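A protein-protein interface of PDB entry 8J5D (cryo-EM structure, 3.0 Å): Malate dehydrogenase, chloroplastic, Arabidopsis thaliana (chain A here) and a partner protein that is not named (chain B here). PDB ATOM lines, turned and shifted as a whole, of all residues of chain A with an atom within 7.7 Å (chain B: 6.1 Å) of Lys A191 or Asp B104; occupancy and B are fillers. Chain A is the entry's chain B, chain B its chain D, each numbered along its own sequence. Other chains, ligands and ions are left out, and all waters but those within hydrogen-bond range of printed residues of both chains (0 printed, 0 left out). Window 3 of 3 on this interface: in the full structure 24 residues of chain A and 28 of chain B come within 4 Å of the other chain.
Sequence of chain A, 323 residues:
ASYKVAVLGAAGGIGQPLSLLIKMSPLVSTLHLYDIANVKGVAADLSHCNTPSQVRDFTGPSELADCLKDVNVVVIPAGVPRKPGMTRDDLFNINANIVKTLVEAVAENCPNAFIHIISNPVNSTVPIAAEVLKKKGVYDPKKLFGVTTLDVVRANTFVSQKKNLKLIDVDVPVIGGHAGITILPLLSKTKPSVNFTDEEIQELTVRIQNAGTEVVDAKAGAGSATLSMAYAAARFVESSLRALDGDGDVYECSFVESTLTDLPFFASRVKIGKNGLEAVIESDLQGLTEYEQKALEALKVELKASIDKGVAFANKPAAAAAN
OD1 of Asp A169 lies within salt-bridge range of NH2 of Arg B109.
The side-chain carboxylate (OD1) of Asp A171 sits close to the backbone carbonyl oxygen (O) of Arg B109, at 3.3 Å.
The side-chain amino group (NZ) of Lys A191 is in salt-bridge range of the side-chain carboxylate (OD1) of Asp B104.
The guanidinium group (NH1) of Arg A269 is in salt-bridge range of the side-chain carboxylate (OD2) of Asp A171, at 2.5 Å.
The backbone NH (N) of Lys A191 lies within hydrogen-bond range of the backbone carbonyl oxygen (O) of Asp A171, at 3.2 Å.
The side-chain carboxylate (OD2) of Asp B104 is in hydrogen-bond range of the side-chain hydroxyl (OG) of Ser B101, 2.7 Å away.
The backbone carbonyl oxygen (O) of Asp B104 lies within hydrogen-bond range of the guanidinium group (NH1) of Arg B109, 3.0 Å away.
Among the printed residues, merely in contact across the chains: Tyr A251 with Asp B102, Lys A191 with Arg B109, Arg A269 with Leu B103, Lys A191 with Leu B103 and Tyr A251 with Leu B103.
Printed residues of chain B within 4 Å of Asp A171: Arg B109 (3.3 Å).
Pro A173 touches none of the printed residues of chain B.
Lys A191 touches just these residues of chain B: Leu B103 (3.7 Å), Asp B104 (2.7 Å) and Arg B109 (3.4 Å).
Pro A192 touches none of the printed residues of chain B.
Of the printed residues of chain B, Tyr A251 touches Asp B102 and Leu B103.
Of the printed residues of chain A, Asp B102 touches Tyr A251.
Of the printed residues of chain A, Leu B103 touches Lys A191, Tyr A251 and Arg A269.
Of chain A, only Lys A191 comes within 4 Å of Asp B104.
The nearest residue of chain A that does not touch Asp B104 is Tyr A251 (6.6 Å).
Printed residues of chain A that touch a printed residue of chain B: Asp A169, Asp A171, Lys A191, Tyr A251 and Arg A269.
Along chain A the printed residues that touch a printed residue of chain B span positions 169 to 269.
Among the printed residues, Asp or Glu carboxylates within 4 Å of a Lys or Arg side-chain nitrogen of the other chain: Asp A169 with Arg B109 and Lys A191 with Asp B104.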
ATOM      1  N   ASN A 156     -11.917 -26.015  19.313  1.00  0.00           N
ATOM      2  CA  ASN A 156     -11.823 -24.956  20.314  1.00  0.00           C
ATOM      3  C   ASN A 156     -11.278 -25.500  21.626  1.00  0.00           C
ATOM      4  O   ASN A 156     -10.341 -24.938  22.205  1.00  0.00           O
ATOM      5  CB  ASN A 156     -13.188 -24.307  20.536  1.00  0.00           C
ATOM      6  CG  ASN A 156     -13.762 -23.707  19.278  1.00  0.00           C
ATOM      7  OD1 ASN A 156     -13.249 -22.716  18.765  1.00  0.00           O
ATOM      8  ND2 ASN A 156     -14.846 -24.284  18.786  1.00  0.00           N
ATOM      9  N   LEU A 165      -5.184 -20.799  26.095  1.00  0.00           N
ATOM     10  CA  LEU A 165      -5.871 -19.650  25.525  1.00  0.00           C
ATOM     11  C   LEU A 165      -7.236 -19.487  26.177  1.00  0.00           C
ATOM     12  O   LEU A 165      -7.829 -20.455  26.661  1.00  0.00           O
ATOM     13  CB  LEU A 165      -6.033 -19.798  24.008  1.00  0.00           C
ATOM     14  CG  LEU A 165      -5.294 -18.789  23.128  1.00  0.00           C
ATOM     15  CD1 LEU A 165      -5.787 -18.876  21.693  1.00  0.00           C
ATOM     16  CD2 LEU A 165      -5.456 -17.378  23.670  1.00  0.00           C
ATOM     17  N   ASP A 169     -12.625 -16.881  23.577  1.00  0.00           N
ATOM     18  CA  ASP A 169     -12.186 -16.188  22.372  1.00  0.00           C
ATOM     19  C   ASP A 169     -11.819 -17.116  21.223  1.00  0.00           C
ATOM     20  O   ASP A 169     -11.915 -16.706  20.063  1.00  0.00           O
ATOM     21  CB  ASP A 169     -10.979 -15.298  22.688  1.00  0.00           C
ATOM     22  CG  ASP A 169     -11.321 -14.168  23.637  1.00  0.00           C
ATOM     23  OD1 ASP A 169     -12.329 -13.472  23.397  1.00  0.00           O
ATOM     24  OD2 ASP A 169     -10.578 -13.974  24.623  1.00  0.00           O
ATOM     25  N   VAL A 170     -11.404 -18.351  21.508  1.00  0.00           N
ATOM     26  CA  VAL A 170     -10.877 -19.224  20.464  1.00  0.00           C
ATOM     27  C   VAL A 170     -11.999 -19.676  19.541  1.00  0.00           C
ATOM     28  O   VAL A 170     -13.054 -20.139  19.994  1.00  0.00           O
ATOM     29  CB  VAL A 170     -10.150 -20.427  21.080  1.00  0.00           C
ATOM     30  CG1 VAL A 170      -9.234 -21.068  20.051  1.00  0.00           C
ATOM     31  CG2 VAL A 170      -9.351 -19.996  22.294  1.00  0.00           C
ATOM     32  N   ASP A 171     -11.773 -19.541  18.234  1.00  0.00           N
ATOM     33  CA  ASP A 171     -12.684 -20.050  17.211  1.00  0.00           C
ATOM     34  C   ASP A 171     -11.840 -20.605  16.073  1.00  0.00           C
ATOM     35  O   ASP A 171     -11.108 -19.855  15.419  1.00  0.00           O
ATOM     36  CB  ASP A 171     -13.632 -18.961  16.709  1.00  0.00           C
ATOM     37  CG  ASP A 171     -14.775 -19.521  15.887  1.00  0.00           C
ATOM     38  OD1 ASP A 171     -15.615 -20.250  16.452  1.00  0.00           O
ATOM     39  OD2 ASP A 171     -14.834 -19.232  14.673  1.00  0.00           O
ATOM     40  N   VAL A 172     -11.936 -21.906  15.839  1.00  0.00           N
ATOM     41  CA  VAL A 172     -11.129 -22.608  14.846  1.00  0.00           C
ATOM     42  C   VAL A 172     -12.053 -23.094  13.734  1.00  0.00           C
ATOM     43  O   VAL A 172     -12.945 -23.911  13.994  1.00  0.00           O
ATOM     44  CB  VAL A 172     -10.359 -23.782  15.470  1.00  0.00           C
ATOM     45  CG1 VAL A 172      -9.494 -24.457  14.422  1.00  0.00           C
ATOM     46  CG2 VAL A 172      -9.514 -23.299  16.635  1.00  0.00           C
ATOM     47  N   PRO A 173     -11.883 -22.631  12.496  1.00  0.00           N
ATOM     48  CA  PRO A 173     -12.710 -23.142  11.399  1.00  0.00           C
ATOM     49  C   PRO A 173     -12.198 -24.479  10.888  1.00  0.00           C
ATOM     50  O   PRO A 173     -10.996 -24.677  10.691  1.00  0.00           O
ATOM     51  CB  PRO A 173     -12.583 -22.052  10.330  1.00  0.00           C
ATOM     52  CG  PRO A 173     -11.231 -21.474  10.565  1.00  0.00           C
ATOM     53  CD  PRO A 173     -10.952 -21.582  12.047  1.00  0.00           C
ATOM     54  N   LEU A 186      -8.463 -25.690  10.104  1.00  0.00           N
ATOM     55  CA  LEU A 186      -7.682 -24.559   9.610  1.00  0.00           C
ATOM     56  C   LEU A 186      -7.151 -23.792  10.818  1.00  0.00           C
ATOM     57  O   LEU A 186      -7.633 -22.717  11.183  1.00  0.00           O
ATOM     58  CB  LEU A 186      -8.525 -23.681   8.695  1.00  0.00           C
ATOM     59  CG  LEU A 186      -9.171 -24.417   7.520  1.00  0.00           C
ATOM     60  CD1 LEU A 186      -9.998 -23.468   6.673  1.00  0.00           C
ATOM     61  CD2 LEU A 186      -8.110 -25.105   6.677  1.00  0.00           C
ATOM     62  N   LEU A 187      -6.130 -24.376  11.450  1.00  0.00           N
ATOM     63  CA  LEU A 187      -5.576 -23.803  12.670  1.00  0.00           C
ATOM     64  C   LEU A 187      -4.961 -22.433  12.422  1.00  0.00           C
ATOM     65  O   LEU A 187      -5.051 -21.548  13.280  1.00  0.00           O
ATOM     66  CB  LEU A 187      -4.541 -24.755  13.270  1.00  0.00           C
ATOM     67  CG  LEU A 187      -5.102 -26.095  13.756  1.00  0.00           C
ATOM     68  CD1 LEU A 187      -3.999 -26.990  14.289  1.00  0.00           C
ATOM     69  CD2 LEU A 187      -6.167 -25.876  14.817  1.00  0.00           C
ATOM     70  N   SER A 188      -4.345 -22.234  11.254  1.00  0.00           N
ATOM     71  CA  SER A 188      -3.774 -20.934  10.925  1.00  0.00           C
ATOM     72  C   SER A 188      -4.833 -19.843  10.842  1.00  0.00           C
ATOM     73  O   SER A 188      -4.490 -18.658  10.912  1.00  0.00           O
ATOM     74  CB  SER A 188      -3.004 -21.014   9.606  1.00  0.00           C
ATOM     75  OG  SER A 188      -1.846 -21.817   9.742  1.00  0.00           O
ATOM     76  N   LYS A 189      -6.106 -20.213  10.695  1.00  0.00           N
ATOM     77  CA  LYS A 189      -7.211 -19.264  10.731  1.00  0.00           C
ATOM     78  C   LYS A 189      -7.862 -19.189  12.107  1.00  0.00           C
ATOM     79  O   LYS A 189      -9.051 -18.868  12.214  1.00  0.00           O
ATOM     80  CB  LYS A 189      -8.257 -19.614   9.674  1.00  0.00           C
ATOM     81  CG  LYS A 189      -7.694 -19.986   8.317  1.00  0.00           C
ATOM     82  CD  LYS A 189      -8.781 -19.924   7.254  1.00  0.00           C
ATOM     83  CE  LYS A 189      -9.743 -18.777   7.529  1.00  0.00           C
ATOM     84  NZ  LYS A 189     -10.880 -18.734   6.577  1.00  0.00           N
ATOM     85  N   THR A 190      -7.111 -19.490  13.164  1.00  0.00           N
ATOM     86  CA  THR A 190      -7.619 -19.312  14.517  1.00  0.00           C
ATOM     87  C   THR A 190      -7.826 -17.826  14.778  1.00  0.00           C
ATOM     88  O   THR A 190      -6.892 -17.030  14.633  1.00  0.00           O
ATOM     89  CB  THR A 190      -6.648 -19.910  15.533  1.00  0.00           C
ATOM     90  OG1 THR A 190      -6.475 -21.306  15.264  1.00  0.00           O
ATOM     91  CG2 THR A 190      -7.180 -19.735  16.944  1.00  0.00           C
ATOM     92  N   LYS A 191      -9.049 -17.452  15.154  1.00  0.00           N
ATOM     93  CA  LYS A 191      -9.382 -16.035  15.273  1.00  0.00           C
ATOM     94  C   LYS A 191      -8.521 -15.298  16.293  1.00  0.00           C
ATOM     95  O   LYS A 191      -8.057 -14.190  15.974  1.00  0.00           O
ATOM     96  CB  LYS A 191     -10.874 -15.880  15.584  1.00  0.00           C
ATOM     97  CG  LYS A 191     -11.789 -16.285  14.442  1.00  0.00           C
ATOM     98  CD  LYS A 191     -11.404 -15.590  13.149  1.00  0.00           C
ATOM     99  CE  LYS A 191     -11.698 -14.101  13.208  1.00  0.00           C
ATOM    100  NZ  LYS A 191     -11.322 -13.412  11.943  1.00  0.00           N
ATOM    101  N   PRO A 192      -8.268 -15.819  17.504  1.00  0.00           N
ATOM    102  CA  PRO A 192      -7.196 -15.237  18.319  1.00  0.00           C
ATOM    103  C   PRO A 192      -5.842 -15.651  17.769  1.00  0.00           C
ATOM    104  O   PRO A 192      -5.260 -16.641  18.220  1.00  0.00           O
ATOM    105  CB  PRO A 192      -7.454 -15.813  19.715  1.00  0.00           C
ATOM    106  CG  PRO A 192      -8.163 -17.081  19.462  1.00  0.00           C
ATOM    107  CD  PRO A 192      -9.020 -16.841  18.254  1.00  0.00           C
ATOM    108  N   SER A 193      -5.359 -14.904  16.774  1.00  0.00           N
ATOM    109  CA  SER A 193      -4.180 -15.281  16.001  1.00  0.00           C
ATOM    110  C   SER A 193      -3.024 -15.687  16.903  1.00  0.00           C
ATOM    111  O   SER A 193      -2.498 -14.871  17.666  1.00  0.00           O
ATOM    112  CB  SER A 193      -3.764 -14.119  15.098  1.00  0.00           C
ATOM    113  OG  SER A 193      -4.017 -12.874  15.725  1.00  0.00           O
ATOM    114  N   VAL A 194      -2.634 -16.954  16.806  1.00  0.00           N
ATOM    115  CA  VAL A 194      -1.573 -17.526  17.623  1.00  0.00           C
ATOM    116  C   VAL A 194      -0.710 -18.412  16.736  1.00  0.00           C
ATOM    117  O   VAL A 194      -1.225 -19.179  15.916  1.00  0.00           O
ATOM    118  CB  VAL A 194      -2.147 -18.318  18.818  1.00  0.00           C
ATOM    119  CG1 VAL A 194      -3.269 -19.240  18.359  1.00  0.00           C
ATOM    120  CG2 VAL A 194      -1.054 -19.103  19.523  1.00  0.00           C
ATOM    121  N   TYR A 251     -22.170 -16.824  11.917  1.00  0.00           N
ATOM    122  CA  TYR A 251     -21.240 -17.590  11.101  1.00  0.00           C
ATOM    123  C   TYR A 251     -21.073 -18.961  11.736  1.00  0.00           C
ATOM    124  O   TYR A 251     -20.877 -19.062  12.952  1.00  0.00           O
ATOM    125  CB  TYR A 251     -19.883 -16.889  10.990  1.00  0.00           C
ATOM    126  CG  TYR A 251     -19.933 -15.521  10.348  1.00  0.00           C
ATOM    127  CD1 TYR A 251     -20.238 -14.393  11.095  1.00  0.00           C
ATOM    128  CD2 TYR A 251     -19.661 -15.357   8.997  1.00  0.00           C
ATOM    129  CE1 TYR A 251     -20.281 -13.141  10.514  1.00  0.00           C
ATOM    130  CE2 TYR A 251     -19.700 -14.110   8.406  1.00  0.00           C
ATOM    131  CZ  TYR A 251     -20.010 -13.005   9.171  1.00  0.00           C
ATOM    132  OH  TYR A 251     -20.051 -11.759   8.589  1.00  0.00           O
ATOM    133  N   ARG A 269     -17.099 -22.660   6.695  1.00  0.00           N
ATOM    134  CA  ARG A 269     -17.763 -21.630   7.482  1.00  0.00           C
ATOM    135  C   ARG A 269     -18.634 -20.791   6.559  1.00  0.00           C
ATOM    136  O   ARG A 269     -18.139 -20.206   5.590  1.00  0.00           O
ATOM    137  CB  ARG A 269     -16.737 -20.760   8.203  1.00  0.00           C
ATOM    138  CG  ARG A 269     -17.220 -19.350   8.502  1.00  0.00           C
ATOM    139  CD  ARG A 269     -16.816 -18.909   9.896  1.00  0.00           C
ATOM    140  NE  ARG A 269     -15.370 -18.791  10.031  1.00  0.00           N
ATOM    141  CZ  ARG A 269     -14.702 -19.004  11.157  1.00  0.00           C
ATOM    142  NH1 ARG A 269     -15.323 -19.354  12.272  1.00  0.00           N
ATOM    143  NH2 ARG A 269     -13.380 -18.862  11.164  1.00  0.00           N
ATOM    144  N   HIS B  99     -13.378  -2.058   8.349  1.00  0.00           N
ATOM    145  CA  HIS B  99     -12.240  -2.966   8.247  1.00  0.00           C
ATOM    146  C   HIS B  99     -12.547  -4.333   8.849  1.00  0.00           C
ATOM    147  O   HIS B  99     -12.538  -5.350   8.147  1.00  0.00           O
ATOM    148  CB  HIS B  99     -11.020  -2.343   8.928  1.00  0.00           C
ATOM    149  CG  HIS B  99      -9.803  -3.215   8.899  1.00  0.00           C
ATOM    150  ND1 HIS B  99      -9.101  -3.476   7.742  1.00  0.00           N
ATOM    151  CD2 HIS B  99      -9.164  -3.886   9.886  1.00  0.00           C
ATOM    152  CE1 HIS B  99      -8.082  -4.270   8.018  1.00  0.00           C
ATOM    153  NE2 HIS B  99      -8.098  -4.534   9.312  1.00  0.00           N
ATOM    154  N   LEU B 100     -12.819  -4.375  10.151  1.00  0.00           N
ATOM    155  CA  LEU B 100     -13.031  -5.640  10.838  1.00  0.00           C
ATOM    156  C   LEU B 100     -14.328  -6.291  10.374  1.00  0.00           C
ATOM    157  O   LEU B 100     -15.353  -5.621  10.222  1.00  0.00           O
ATOM    158  CB  LEU B 100     -13.060  -5.420  12.348  1.00  0.00           C
ATOM    159  CG  LEU B 100     -11.819  -4.762  12.954  1.00  0.00           C
ATOM    160  CD1 LEU B 100     -12.015  -4.517  14.440  1.00  0.00           C
ATOM    161  CD2 LEU B 100     -10.583  -5.608  12.706  1.00  0.00           C
ATOM    162  N   SER B 101     -14.276  -7.600  10.149  1.00  0.00           N
ATOM    163  CA  SER B 101     -15.453  -8.354   9.751  1.00  0.00           C
ATOM    164  C   SER B 101     -16.359  -8.597  10.954  1.00  0.00           C
ATOM    165  O   SER B 101     -15.964  -8.420  12.110  1.00  0.00           O
ATOM    166  CB  SER B 101     -15.051  -9.684   9.115  1.00  0.00           C
ATOM    167  OG  SER B 101     -14.361 -10.503  10.041  1.00  0.00           O
ATOM    168  N   ASP B 102     -17.596  -9.009  10.665  1.00  0.00           N
ATOM    169  CA  ASP B 102     -18.559  -9.250  11.734  1.00  0.00           C
ATOM    170  C   ASP B 102     -18.107 -10.376  12.655  1.00  0.00           C
ATOM    171  O   ASP B 102     -18.510 -10.421  13.822  1.00  0.00           O
ATOM    172  CB  ASP B 102     -19.935  -9.563  11.143  1.00  0.00           C
ATOM    173  CG  ASP B 102     -20.695  -8.310  10.745  1.00  0.00           C
ATOM    174  OD1 ASP B 102     -20.291  -7.207  11.164  1.00  0.00           O
ATOM    175  OD2 ASP B 102     -21.700  -8.430  10.013  1.00  0.00           O
ATOM    176  N   LEU B 103     -17.274 -11.290  12.153  1.00  0.00           N
ATOM    177  CA  LEU B 103     -16.727 -12.337  13.008  1.00  0.00           C
ATOM    178  C   LEU B 103     -15.642 -11.788  13.927  1.00  0.00           C
ATOM    179  O   LEU B 103     -15.497 -12.243  15.068  1.00  0.00           O
ATOM    180  CB  LEU B 103     -16.183 -13.481  12.154  1.00  0.00           C
ATOM    181  CG  LEU B 103     -15.436 -14.600  12.884  1.00  0.00           C
ATOM    182  CD1 LEU B 103     -16.347 -15.293  13.884  1.00  0.00           C
ATOM    183  CD2 LEU B 103     -14.866 -15.598  11.890  1.00  0.00           C
ATOM    184  N   ASP B 104     -14.867 -10.813  13.446  1.00  0.00           N
ATOM    185  CA  ASP B 104     -13.820 -10.220  14.273  1.00  0.00           C
ATOM    186  C   ASP B 104     -14.406  -9.516  15.489  1.00  0.00           C
ATOM    187  O   ASP B 104     -13.876  -9.631  16.600  1.00  0.00           O
ATOM    188  CB  ASP B 104     -12.985  -9.244  13.446  1.00  0.00           C
ATOM    189  CG  ASP B 104     -12.068  -9.944  12.465  1.00  0.00           C
ATOM    190  OD1 ASP B 104     -11.322 -10.850  12.892  1.00  0.00           O
ATOM    191  OD2 ASP B 104     -12.091  -9.586  11.269  1.00  0.00           O
ATOM    192  N   LEU B 105     -15.498  -8.777  15.299  1.00  0.00           N
ATOM    193  CA  LEU B 105     -16.133  -8.036  16.389  1.00  0.00           C
ATOM    194  C   LEU B 105     -17.272  -8.867  16.979  1.00  0.00           C
ATOM    195  O   LEU B 105     -18.458  -8.558  16.845  1.00  0.00           O
ATOM    196  CB  LEU B 105     -16.619  -6.681  15.895  1.00  0.00           C
ATOM    197  CG  LEU B 105     -15.533  -5.679  15.502  1.00  0.00           C
ATOM    198  CD1 LEU B 105     -16.119  -4.551  14.672  1.00  0.00           C
ATOM    199  CD2 LEU B 105     -14.846  -5.133  16.744  1.00  0.00           C
ATOM    200  N   LEU B 106     -16.882  -9.950  17.647  1.00  0.00           N
ATOM    201  CA  LEU B 106     -17.818 -10.830  18.327  1.00  0.00           C
ATOM    202  C   LEU B 106     -17.326 -11.091  19.741  1.00  0.00           C
ATOM    203  O   LEU B 106     -16.121 -11.154  19.996  1.00  0.00           O
ATOM    204  CB  LEU B 106     -17.995 -12.158  17.581  1.00  0.00           C
ATOM    205  CG  LEU B 106     -19.415 -12.728  17.537  1.00  0.00           C
ATOM    206  CD1 LEU B 106     -20.445 -11.618  17.408  1.00  0.00           C
ATOM    207  CD2 LEU B 106     -19.555 -13.725  16.399  1.00  0.00           C
ATOM    208  N   ARG B 109     -17.127 -15.772  20.518  1.00  0.00           N
ATOM    209  CA  ARG B 109     -16.689 -16.342  19.249  1.00  0.00           C
ATOM    210  C   ARG B 109     -16.789 -17.860  19.287  1.00  0.00           C
ATOM    211  O   ARG B 109     -17.522 -18.470  18.500  1.00  0.00           O
ATOM    212  CB  ARG B 109     -15.265 -15.890  18.942  1.00  0.00           C
ATOM    213  CG  ARG B 109     -15.141 -15.144  17.634  1.00  0.00           C
ATOM    214  CD  ARG B 109     -13.693 -14.922  17.283  1.00  0.00           C
ATOM    215  NE  ARG B 109     -12.920 -14.441  18.422  1.00  0.00           N
ATOM    216  CZ  ARG B 109     -12.725 -13.162  18.707  1.00  0.00           C
ATOM    217  NH1 ARG B 109     -13.234 -12.202  17.955  1.00  0.00           N
ATOM    218  NH2 ARG B 109     -11.999 -12.839  19.774  1.00  0.00           N
